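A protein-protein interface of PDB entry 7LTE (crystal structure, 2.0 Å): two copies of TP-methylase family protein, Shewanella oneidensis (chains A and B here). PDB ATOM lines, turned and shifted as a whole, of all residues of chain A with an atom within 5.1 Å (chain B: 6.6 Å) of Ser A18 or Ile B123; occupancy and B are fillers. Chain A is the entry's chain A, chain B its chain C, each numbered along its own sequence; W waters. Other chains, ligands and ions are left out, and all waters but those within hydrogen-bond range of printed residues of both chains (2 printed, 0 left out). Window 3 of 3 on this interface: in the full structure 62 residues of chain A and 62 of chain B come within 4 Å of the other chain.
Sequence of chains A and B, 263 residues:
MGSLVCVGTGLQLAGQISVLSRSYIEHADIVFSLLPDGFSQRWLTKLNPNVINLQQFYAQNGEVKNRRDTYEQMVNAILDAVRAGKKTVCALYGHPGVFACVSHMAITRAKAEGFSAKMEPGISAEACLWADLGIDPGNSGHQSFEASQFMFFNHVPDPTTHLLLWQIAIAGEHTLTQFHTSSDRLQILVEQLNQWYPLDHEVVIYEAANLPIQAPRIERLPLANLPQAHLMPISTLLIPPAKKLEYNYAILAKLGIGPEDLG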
ATOM      1  N   GLY A   8     -13.161   3.177 -10.672  1.00  0.00           N
ATOM      2  CA  GLY A   8     -13.759   4.345 -11.315  1.00  0.00           C
ATOM      3  C   GLY A   8     -12.918   5.578 -11.082  1.00  0.00           C
ATOM      4  O   GLY A   8     -12.286   5.656 -10.069  1.00  0.00           O
ATOM      5  N   GLN A  16     -11.709  13.308  -8.352  1.00  0.00           N
ATOM      6  CA  GLN A  16     -12.960  12.615  -7.987  1.00  0.00           C
ATOM      7  C   GLN A  16     -12.712  11.094  -7.933  1.00  0.00           C
ATOM      8  O   GLN A  16     -13.663  10.331  -7.676  1.00  0.00           O
ATOM      9  CB  GLN A  16     -14.095  12.986  -8.939  1.00  0.00           C
ATOM     10  CG  GLN A  16     -15.485  12.701  -8.364  1.00  0.00           C
ATOM     11  CD  GLN A  16     -16.559  13.509  -9.045  1.00  0.00           C
ATOM     12  OE1 GLN A  16     -16.765  13.381 -10.258  1.00  0.00           O
ATOM     13  NE2 GLN A  16     -17.121  14.450  -8.284  1.00  0.00           N
ATOM     14  N   ILE A  17     -11.462  10.661  -8.128  1.00  0.00           N
ATOM     15  CA  ILE A  17     -11.100   9.244  -7.847  1.00  0.00           C
ATOM     16  C   ILE A  17     -10.928   9.080  -6.330  1.00  0.00           C
ATOM     17  O   ILE A  17     -10.365  10.020  -5.662  1.00  0.00           O
ATOM     18  CB  ILE A  17      -9.862   8.829  -8.674  1.00  0.00           C
ATOM     19  CG1 ILE A  17      -9.615   7.315  -8.618  1.00  0.00           C
ATOM     20  CG2 ILE A  17      -8.615   9.633  -8.327  1.00  0.00           C
ATOM     21  CD1 ILE A  17      -8.723   6.808  -9.750  1.00  0.00           C
ATOM     22  N   SER A  18     -11.247   7.900  -5.802  1.00  0.00           N
ATOM     23  CA  SER A  18     -10.923   7.474  -4.405  1.00  0.00           C
ATOM     24  C   SER A  18      -9.399   7.430  -4.204  1.00  0.00           C
ATOM     25  O   SER A  18      -8.705   7.114  -5.164  1.00  0.00           O
ATOM     26  CB  SER A  18     -11.514   6.116  -4.095  1.00  0.00           C
ATOM     27  OG  SER A  18     -12.937   6.157  -4.234  1.00  0.00           O
ATOM     28  N   VAL A  19      -8.919   7.714  -2.994  1.00  0.00           N
ATOM     29  CA  VAL A  19      -7.478   7.580  -2.622  1.00  0.00           C
ATOM     30  C   VAL A  19      -6.971   6.156  -2.966  1.00  0.00           C
ATOM     31  O   VAL A  19      -5.836   6.014  -3.561  1.00  0.00           O
ATOM     32  CB  VAL A  19      -7.283   7.904  -1.129  1.00  0.00           C
ATOM     33  CG1 VAL A  19      -5.896   7.549  -0.624  1.00  0.00           C
ATOM     34  CG2 VAL A  19      -7.579   9.392  -0.868  1.00  0.00           C
ATOM     35  N   LEU A  20      -7.700   5.137  -2.518  1.00  0.00           N
ATOM     36  CA  LEU A  20      -7.251   3.729  -2.754  1.00  0.00           C
ATOM     37  C   LEU A  20      -7.274   3.440  -4.267  1.00  0.00           C
ATOM     38  O   LEU A  20      -6.328   2.715  -4.780  1.00  0.00           O
ATOM     39  CB  LEU A  20      -8.153   2.772  -1.989  1.00  0.00           C
ATOM     40  CG  LEU A  20      -7.888   1.281  -2.283  1.00  0.00           C
ATOM     41  CD1 LEU A  20      -6.466   0.905  -1.967  1.00  0.00           C
ATOM     42  CD2 LEU A  20      -8.850   0.372  -1.532  1.00  0.00           C
ATOM     43  N   SER A  21      -8.334   3.869  -4.974  1.00  0.00           N
ATOM     44  CA  SER A  21      -8.490   3.575  -6.435  1.00  0.00           C
ATOM     45  C   SER A  21      -7.303   4.163  -7.226  1.00  0.00           C
ATOM     46  O   SER A  21      -6.764   3.440  -8.174  1.00  0.00           O
ATOM     47  CB  SER A  21      -9.801   4.044  -6.969  1.00  0.00           C
ATOM     48  OG  SER A  21     -10.843   3.252  -6.456  1.00  0.00           O
ATOM     49  N   ARG A  22      -6.871   5.377  -6.862  1.00  0.00           N
ATOM     50  CA  ARG A  22      -5.693   6.026  -7.469  1.00  0.00           C
ATOM     51  C   ARG A  22      -4.444   5.142  -7.245  1.00  0.00           C
ATOM     52  O   ARG A  22      -3.661   4.997  -8.187  1.00  0.00           O
ATOM     53  CB  ARG A  22      -5.497   7.427  -6.862  1.00  0.00           C
ATOM     54  CG  ARG A  22      -4.491   8.270  -7.638  1.00  0.00           C
ATOM     55  CD  ARG A  22      -4.268   9.624  -6.987  1.00  0.00           C
ATOM     56  NE  ARG A  22      -3.464  10.501  -7.813  1.00  0.00           N
ATOM     57  CZ  ARG A  22      -2.109  10.546  -7.820  1.00  0.00           C
ATOM     58  NH1 ARG A  22      -1.391   9.705  -7.089  1.00  0.00           N
ATOM     59  NH2 ARG A  22      -1.483  11.429  -8.582  1.00  0.00           N
ATOM     60  N   PRO A 121     -15.967   0.534  -5.923  1.00  0.00           N
ATOM     61  CA  PRO A 121     -16.992   1.522  -6.238  1.00  0.00           C
ATOM     62  C   PRO A 121     -16.352   2.867  -6.595  1.00  0.00           C
ATOM     63  O   PRO A 121     -15.259   3.133  -6.113  1.00  0.00           O
ATOM     64  CB  PRO A 121     -17.824   1.659  -4.939  1.00  0.00           C
ATOM     65  CG  PRO A 121     -17.039   0.965  -3.869  1.00  0.00           C
ATOM     66  CD  PRO A 121     -16.086   0.009  -4.558  1.00  0.00           C
ATOM     67  N   GLY A 122     -17.087   3.708  -7.334  1.00  0.00           N
ATOM     68  CA  GLY A 122     -16.666   5.082  -7.661  1.00  0.00           C
ATOM     69  C   GLY A 122     -17.853   6.022  -7.653  1.00  0.00           C
ATOM     70  O   GLY A 122     -19.013   5.538  -7.410  1.00  0.00           O
ATOM     71  N   ILE A 123     -17.590   7.303  -7.893  1.00  0.00           N
ATOM     72  CA  ILE A 123     -18.625   8.382  -7.907  1.00  0.00           C
ATOM     73  C   ILE A 123     -19.227   8.428  -9.309  1.00  0.00           C
ATOM     74  O   ILE A 123     -18.476   8.723 -10.276  1.00  0.00           O
ATOM     75  CB  ILE A 123     -18.041   9.722  -7.447  1.00  0.00           C
ATOM     76  CG1 ILE A 123     -17.602   9.652  -5.973  1.00  0.00           C
ATOM     77  CG2 ILE A 123     -18.979  10.868  -7.694  1.00  0.00           C
ATOM     78  CD1 ILE A 123     -16.569  10.663  -5.609  1.00  0.00           C
ATOM     79  N   GLY B   8     -18.268  13.736   1.409  1.00  0.00           N
ATOM     80  CA  GLY B   8     -18.470  12.379   1.905  1.00  0.00           C
ATOM     81  C   GLY B   8     -17.147  11.680   2.110  1.00  0.00           C
ATOM     82  O   GLY B   8     -16.172  12.026   1.419  1.00  0.00           O
ATOM     83  N   THR B   9     -17.102  10.748   3.040  1.00  0.00           N
ATOM     84  CA  THR B   9     -15.848  10.005   3.347  1.00  0.00           C
ATOM     85  C   THR B   9     -15.911   8.588   2.781  1.00  0.00           C
ATOM     86  O   THR B   9     -14.913   7.821   2.966  1.00  0.00           O
ATOM     87  CB  THR B   9     -15.552  10.093   4.837  1.00  0.00           C
ATOM     88  OG1 THR B   9     -16.572   9.419   5.556  1.00  0.00           O
ATOM     89  CG2 THR B   9     -15.437  11.550   5.270  1.00  0.00           C
ATOM     90  N   GLY B  10     -17.046   8.222   2.191  1.00  0.00           N
ATOM     91  CA  GLY B  10     -17.233   6.870   1.675  1.00  0.00           C
ATOM     92  C   GLY B  10     -17.526   5.976   2.858  1.00  0.00           C
ATOM     93  O   GLY B  10     -17.793   6.545   3.968  1.00  0.00           O
ATOM     94  N   LEU B  11     -17.591   4.661   2.622  1.00  0.00           N
ATOM     95  CA  LEU B  11     -17.941   3.655   3.672  1.00  0.00           C
ATOM     96  C   LEU B  11     -16.674   3.086   4.296  1.00  0.00           C
ATOM     97  O   LEU B  11     -16.608   2.932   5.543  1.00  0.00           O
ATOM     98  CB  LEU B  11     -18.787   2.535   3.058  1.00  0.00           C
ATOM     99  CG  LEU B  11     -20.291   2.820   3.057  1.00  0.00           C
ATOM    100  CD1 LEU B  11     -20.881   2.842   4.451  1.00  0.00           C
ATOM    101  CD2 LEU B  11     -20.551   4.118   2.348  1.00  0.00           C
ATOM    102  N   GLY B  15      -9.518   5.312   2.629  1.00  0.00           N
ATOM    103  CA  GLY B  15      -9.238   5.106   1.192  1.00  0.00           C
ATOM    104  C   GLY B  15     -10.390   5.418   0.242  1.00  0.00           C
ATOM    105  O   GLY B  15     -10.129   5.581  -0.991  1.00  0.00           O
ATOM    106  N   GLN B  16     -11.616   5.490   0.738  1.00  0.00           N
ATOM    107  CA  GLN B  16     -12.803   5.606  -0.148  1.00  0.00           C
ATOM    108  C   GLN B  16     -13.256   7.085  -0.279  1.00  0.00           C
ATOM    109  O   GLN B  16     -14.220   7.327  -1.012  1.00  0.00           O
ATOM    110  CB  GLN B  16     -13.914   4.701   0.356  1.00  0.00           C
ATOM    111  CG  GLN B  16     -14.951   4.425  -0.675  1.00  0.00           C
ATOM    112  CD  GLN B  16     -15.702   3.149  -0.360  1.00  0.00           C
ATOM    113  OE1 GLN B  16     -16.402   3.063   0.646  1.00  0.00           O
ATOM    114  NE2 GLN B  16     -15.466   2.122  -1.158  1.00  0.00           N
ATOM    115  N   ILE B  17     -12.547   8.028   0.362  1.00  0.00           N
ATOM    116  CA  ILE B  17     -12.744   9.494   0.121  1.00  0.00           C
ATOM    117  C   ILE B  17     -12.114   9.871  -1.229  1.00  0.00           C
ATOM    118  O   ILE B  17     -11.050   9.299  -1.604  1.00  0.00           O
ATOM    119  CB  ILE B  17     -12.215  10.330   1.306  1.00  0.00           C
ATOM    120  CG1 ILE B  17     -12.664  11.788   1.208  1.00  0.00           C
ATOM    121  CG2 ILE B  17     -10.698  10.200   1.462  1.00  0.00           C
ATOM    122  CD1 ILE B  17     -12.471  12.577   2.500  1.00  0.00           C
ATOM    123  N   SER B  18     -12.692  10.838  -1.945  1.00  0.00           N
ATOM    124  CA  SER B  18     -12.077  11.403  -3.167  1.00  0.00           C
ATOM    125  C   SER B  18     -10.827  12.226  -2.794  1.00  0.00           C
ATOM    126  O   SER B  18     -10.745  12.817  -1.682  1.00  0.00           O
ATOM    127  CB  SER B  18     -13.033  12.216  -3.978  1.00  0.00           C
ATOM    128  OG  SER B  18     -13.258  13.462  -3.351  1.00  0.00           O
ATOM    129  N   VAL B  19      -9.881  12.319  -3.719  1.00  0.00           N
ATOM    130  CA  VAL B  19      -8.645  13.112  -3.533  1.00  0.00           C
ATOM    131  C   VAL B  19      -8.976  14.571  -3.178  1.00  0.00           C
ATOM    132  O   VAL B  19      -8.385  15.042  -2.173  1.00  0.00           O
ATOM    133  CB  VAL B  19      -7.747  13.048  -4.777  1.00  0.00           C
ATOM    134  CG1 VAL B  19      -6.534  13.959  -4.637  1.00  0.00           C
ATOM    135  CG2 VAL B  19      -7.266  11.607  -4.992  1.00  0.00           C
ATOM    136  N   TYR B  93     -20.311  10.363   6.354  1.00  0.00           N
ATOM    137  CA  TYR B  93     -19.886   9.064   5.766  1.00  0.00           C
ATOM    138  C   TYR B  93     -20.686   8.862   4.457  1.00  0.00           C
ATOM    139  O   TYR B  93     -21.789   9.417   4.284  1.00  0.00           O
ATOM    140  CB  TYR B  93     -20.084   7.947   6.787  1.00  0.00           C
ATOM    141  CG  TYR B  93     -21.513   7.491   6.917  1.00  0.00           C
ATOM    142  CD1 TYR B  93     -22.364   8.089   7.830  1.00  0.00           C
ATOM    143  CD2 TYR B  93     -22.000   6.417   6.195  1.00  0.00           C
ATOM    144  CE1 TYR B  93     -23.685   7.674   7.968  1.00  0.00           C
ATOM    145  CE2 TYR B  93     -23.325   5.976   6.325  1.00  0.00           C
ATOM    146  CZ  TYR B  93     -24.159   6.609   7.217  1.00  0.00           C
ATOM    147  OH  TYR B  93     -25.407   6.115   7.408  1.00  0.00           O
ATOM    148  N   GLY B  94     -20.148   8.052   3.549  1.00  0.00           N
ATOM    149  CA  GLY B  94     -20.730   7.728   2.225  1.00  0.00           C
ATOM    150  C   GLY B  94     -20.774   8.950   1.308  1.00  0.00           C
ATOM    151  O   GLY B  94     -19.755   9.652   1.211  1.00  0.00           O
ATOM    152  N   HIS B  95     -21.954   9.267   0.784  1.00  0.00           N
ATOM    153  CA  HIS B  95     -22.284  10.486   0.003  1.00  0.00           C
ATOM    154  C   HIS B  95     -23.092  11.402   0.916  1.00  0.00           C
ATOM    155  O   HIS B  95     -24.120  10.950   1.459  1.00  0.00           O
ATOM    156  CB  HIS B  95     -23.075  10.051  -1.246  1.00  0.00           C
ATOM    157  CG  HIS B  95     -23.457  11.150  -2.191  1.00  0.00           C
ATOM    158  ND1 HIS B  95     -23.990  12.346  -1.773  1.00  0.00           N
ATOM    159  CD2 HIS B  95     -23.401  11.198  -3.551  1.00  0.00           C
ATOM    160  CE1 HIS B  95     -24.192  13.122  -2.823  1.00  0.00           C
ATOM    161  NE2 HIS B  95     -23.849  12.419  -3.946  1.00  0.00           N
ATOM    162  N   PRO B  96     -22.684  12.686   1.085  1.00  0.00           N
ATOM    163  CA  PRO B  96     -23.292  13.565   2.082  1.00  0.00           C
ATOM    164  C   PRO B  96     -24.757  13.913   1.810  1.00  0.00           C
ATOM    165  O   PRO B  96     -25.492  14.362   2.749  1.00  0.00           O
ATOM    166  CB  PRO B  96     -22.399  14.809   2.032  1.00  0.00           C
ATOM    167  CG  PRO B  96     -21.900  14.858   0.635  1.00  0.00           C
ATOM    168  CD  PRO B  96     -21.688  13.399   0.261  1.00  0.00           C
ATOM    169  N   PRO B 121     -20.008  15.200  -4.220  1.00  0.00           N
ATOM    170  CA  PRO B 121     -20.535  13.836  -4.178  1.00  0.00           C
ATOM    171  C   PRO B 121     -19.480  12.907  -3.558  1.00  0.00           C
ATOM    172  O   PRO B 121     -18.308  13.224  -3.699  1.00  0.00           O
ATOM    173  CB  PRO B 121     -20.815  13.487  -5.649  1.00  0.00           C
ATOM    174  CG  PRO B 121     -19.926  14.437  -6.444  1.00  0.00           C
ATOM    175  CD  PRO B 121     -19.821  15.700  -5.594  1.00  0.00           C
ATOM    176  N   GLY B 122     -19.942  11.786  -2.974  1.00  0.00           N
ATOM    177  CA  GLY B 122     -19.091  10.741  -2.372  1.00  0.00           C
ATOM    178  C   GLY B 122     -19.601   9.365  -2.746  1.00  0.00           C
ATOM    179  O   GLY B 122     -20.639   9.261  -3.466  1.00  0.00           O
ATOM    180  N   ILE B 123     -18.938   8.325  -2.275  1.00  0.00           N
ATOM    181  CA  ILE B 123     -19.330   6.916  -2.596  1.00  0.00           C
ATOM    182  C   ILE B 123     -20.302   6.447  -1.528  1.00  0.00           C
ATOM    183  O   ILE B 123     -19.859   6.366  -0.363  1.00  0.00           O
ATOM    184  CB  ILE B 123     -18.105   6.002  -2.718  1.00  0.00           C
ATOM    185  CG1 ILE B 123     -17.338   6.289  -4.004  1.00  0.00           C
ATOM    186  CG2 ILE B 123     -18.484   4.554  -2.647  1.00  0.00           C
ATOM    187  CD1 ILE B 123     -15.819   6.064  -3.908  1.00  0.00           C
ATOM    188  N   SER B 124     -21.571   6.213  -1.927  1.00  0.00           N
ATOM    189  CA  SER B 124     -22.681   5.851  -1.020  1.00  0.00           C
ATOM    190  C   SER B 124     -22.671   4.343  -0.758  1.00  0.00           C
ATOM    191  O   SER B 124     -22.004   3.576  -1.523  1.00  0.00           O
ATOM    192  CB  SER B 124     -24.025   6.339  -1.588  1.00  0.00           C
ATOM    193  OG  SER B 124     -24.386   5.549  -2.697  1.00  0.00           O
ATOM    194  N   ALA B 125     -23.468   3.895   0.202  1.00  0.00           N
ATOM    195  CA  ALA B 125     -23.690   2.458   0.491  1.00  0.00           C
ATOM    196  C   ALA B 125     -24.248   1.737  -0.762  1.00  0.00           C
ATOM    197  O   ALA B 125     -23.877   0.530  -0.981  1.00  0.00           O
ATOM    198  CB  ALA B 125     -24.626   2.344   1.652  1.00  0.00           C
ATOM    199  N   GLU B 126     -25.088   2.407  -1.559  1.00  0.00           N
ATOM    200  CA  GLU B 126     -25.663   1.866  -2.831  1.00  0.00           C
ATOM    201  C   GLU B 126     -24.541   1.602  -3.847  1.00  0.00           C
ATOM    202  O   GLU B 126     -24.524   0.554  -4.497  1.00  0.00           O
ATOM    203  CB  GLU B 126     -26.660   2.893  -3.362  1.00  0.00           C
ATOM    204  CG  GLU B 126     -26.882   2.865  -4.856  1.00  0.00           C
ATOM    205  CD  GLU B 126     -27.949   3.847  -5.332  1.00  0.00           C
ATOM    206  OE1 GLU B 126     -29.039   3.856  -4.725  1.00  0.00           O
ATOM    207  OE2 GLU B 126     -27.692   4.594  -6.335  1.00  0.00           O
ATOM    208  N   ALA B 127     -23.610   2.535  -3.984  1.00  0.00           N
ATOM    209  CA  ALA B 127     -22.399   2.376  -4.831  1.00  0.00           C
ATOM    210  C   ALA B 127     -21.600   1.126  -4.414  1.00  0.00           C
ATOM    211  O   ALA B 127     -21.139   0.321  -5.339  1.00  0.00           O
ATOM    212  CB  ALA B 127     -21.574   3.636  -4.767  1.00  0.00           C
ATOM    213  N   CYS B 128     -21.454   0.907  -3.107  1.00  0.00           N
ATOM    214  CA  CYS B 128     -20.750  -0.264  -2.569  1.00  0.00           C
ATOM    215  C   CYS B 128     -21.487  -1.551  -2.861  1.00  0.00           C
ATOM    216  O   CYS B 128     -20.807  -2.542  -3.178  1.00  0.00           O
ATOM    217  CB  CYS B 128     -20.536  -0.123  -1.071  1.00  0.00           C
ATOM    218  SG  CYS B 128     -19.404   1.223  -0.621  1.00  0.00           S
HETATM  219  O   HOH W   1     -16.837  14.675  -5.240  1.00  0.00           O
HETATM  220  O   HOH W   2     -13.712   2.191  -3.821  1.00  0.00           O
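Hydrophobic or aromatic side chains of chain B within 4 Å of the printed part of chain A: Ile B17, Val B19, Pro B121 and Ile B123.
Among the printed residues, 17 pairs touch across the chains.
Among the printed residues, no Asp or Glu carboxylate lies within 4 Å of a Lys or Arg side-chain nitrogen of the other chain.
Of the printed residues of chain B, Ser A18 touches Gly B15 (3.4 Å), Gln B16 (3.7 Å), Ile B17 (3.3 Å) and Ile B123 (2.9 Å).
Printed residues of chain B within 4 Å of Val A19: Gly B15 (3.2 Å) and Ile B17 (3.0 Å).
Of the printed residues of chain B, Gly A122 touches Ile B123 (3.7 Å).
Leu B11 touches none of the printed residues of chain A.
Of the printed residues of chain A, Gln B16 touches Ser A18 and Pro A121.
Printed residues of chain A within 4 Å of Ile B123: Ser A18, Pro A121, Gly A122 and Ile A123.
Ala B125 touches none of the printed residues of chain A.
The nearest printed residue of chain B that does not touch Ser A18 is Ser B18 (4.3 Å).
The nearest printed residue of chain A that does not touch Ile B123 is Gln A16 (6.1 Å).
The nearest printed residue of chain A that does not touch Gly B15 is Ser A21 (4.7 Å).
The backbone carbonyl oxygen of Ile A17 lies within hydrogen-bond range of the backbone NH of Val B19 (3.0 Å).
N of Leu A20 sits at hydrogen-bond distance from O of Gly B15, 2.9 Å away.
The backbone carbonyl oxygen (O) of Ile B17 lies within hydrogen-bond range of the backbone NH (N) of Val A19 (3.0 Å).
The backbone carbonyl oxygen (O) of Gly B15 sits at hydrogen-bond distance from the backbone NH (N) of Val A19, 3.2 Å away.
OG of Ser B124 sits at hydrogen-bond distance from N of Ala B127 (3.4 Å).
The side-chain amide oxygen (OE1) of Gln B16 is in hydrogen-bond range of the backbone NH (N) of Leu B11 (2.8 Å).
The side-chain sulfur of Cys B128 lies within hydrogen-bond range of the side-chain amide oxygen of Gln B16 (3.7 Å).
Water W1 bridges the backbone carbonyl oxygen (O) of Pro B121 (2.6 Å) and the side-chain amide nitrogen (NE2) of Gln A16 (3.1 Å).
Water W2 lies within hydrogen-bond range of the backbone carbonyl oxygen (O) of Pro A121 and the side-chain amide nitrogen (NE2) of Gln B16.
Gln A16 touches Pro B121, and with the chains exchanged Pro A121 touches Gln B16.
Ile A17 touches Ser B18, and with the chains exchanged Ser A18 touches Ile B17.
Ser A18 touches Ile B123, but with the chains exchanged Ile A123 does not touch Ser B18 (4.2 Å).
Ile B123 touches its own counterpart, Ile A123.
8 positions are printed for both chains.
Gln A16 touches Pro B121.
Ile A17 touches Ser B18 (O to CA, 3.3 Å).
Gln B16 touches Ser A18.
O of Ile B17 touches CA of Ser A18, at 3.3 Å.
Ile B123 touches Ser A18 (CD1 to OG, 2.9 Å).
CG of Pro A121 touches NE2 of Gln B16, 3.3 Å away.
CB of Pro A121 touches O of Ala B127 (3.6 Å).
Gly A122 touches Ile B123 (C to CG1, 3.7 Å).
Ile A123 touches Gly B122.
Ile A123 touches Ile B123.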
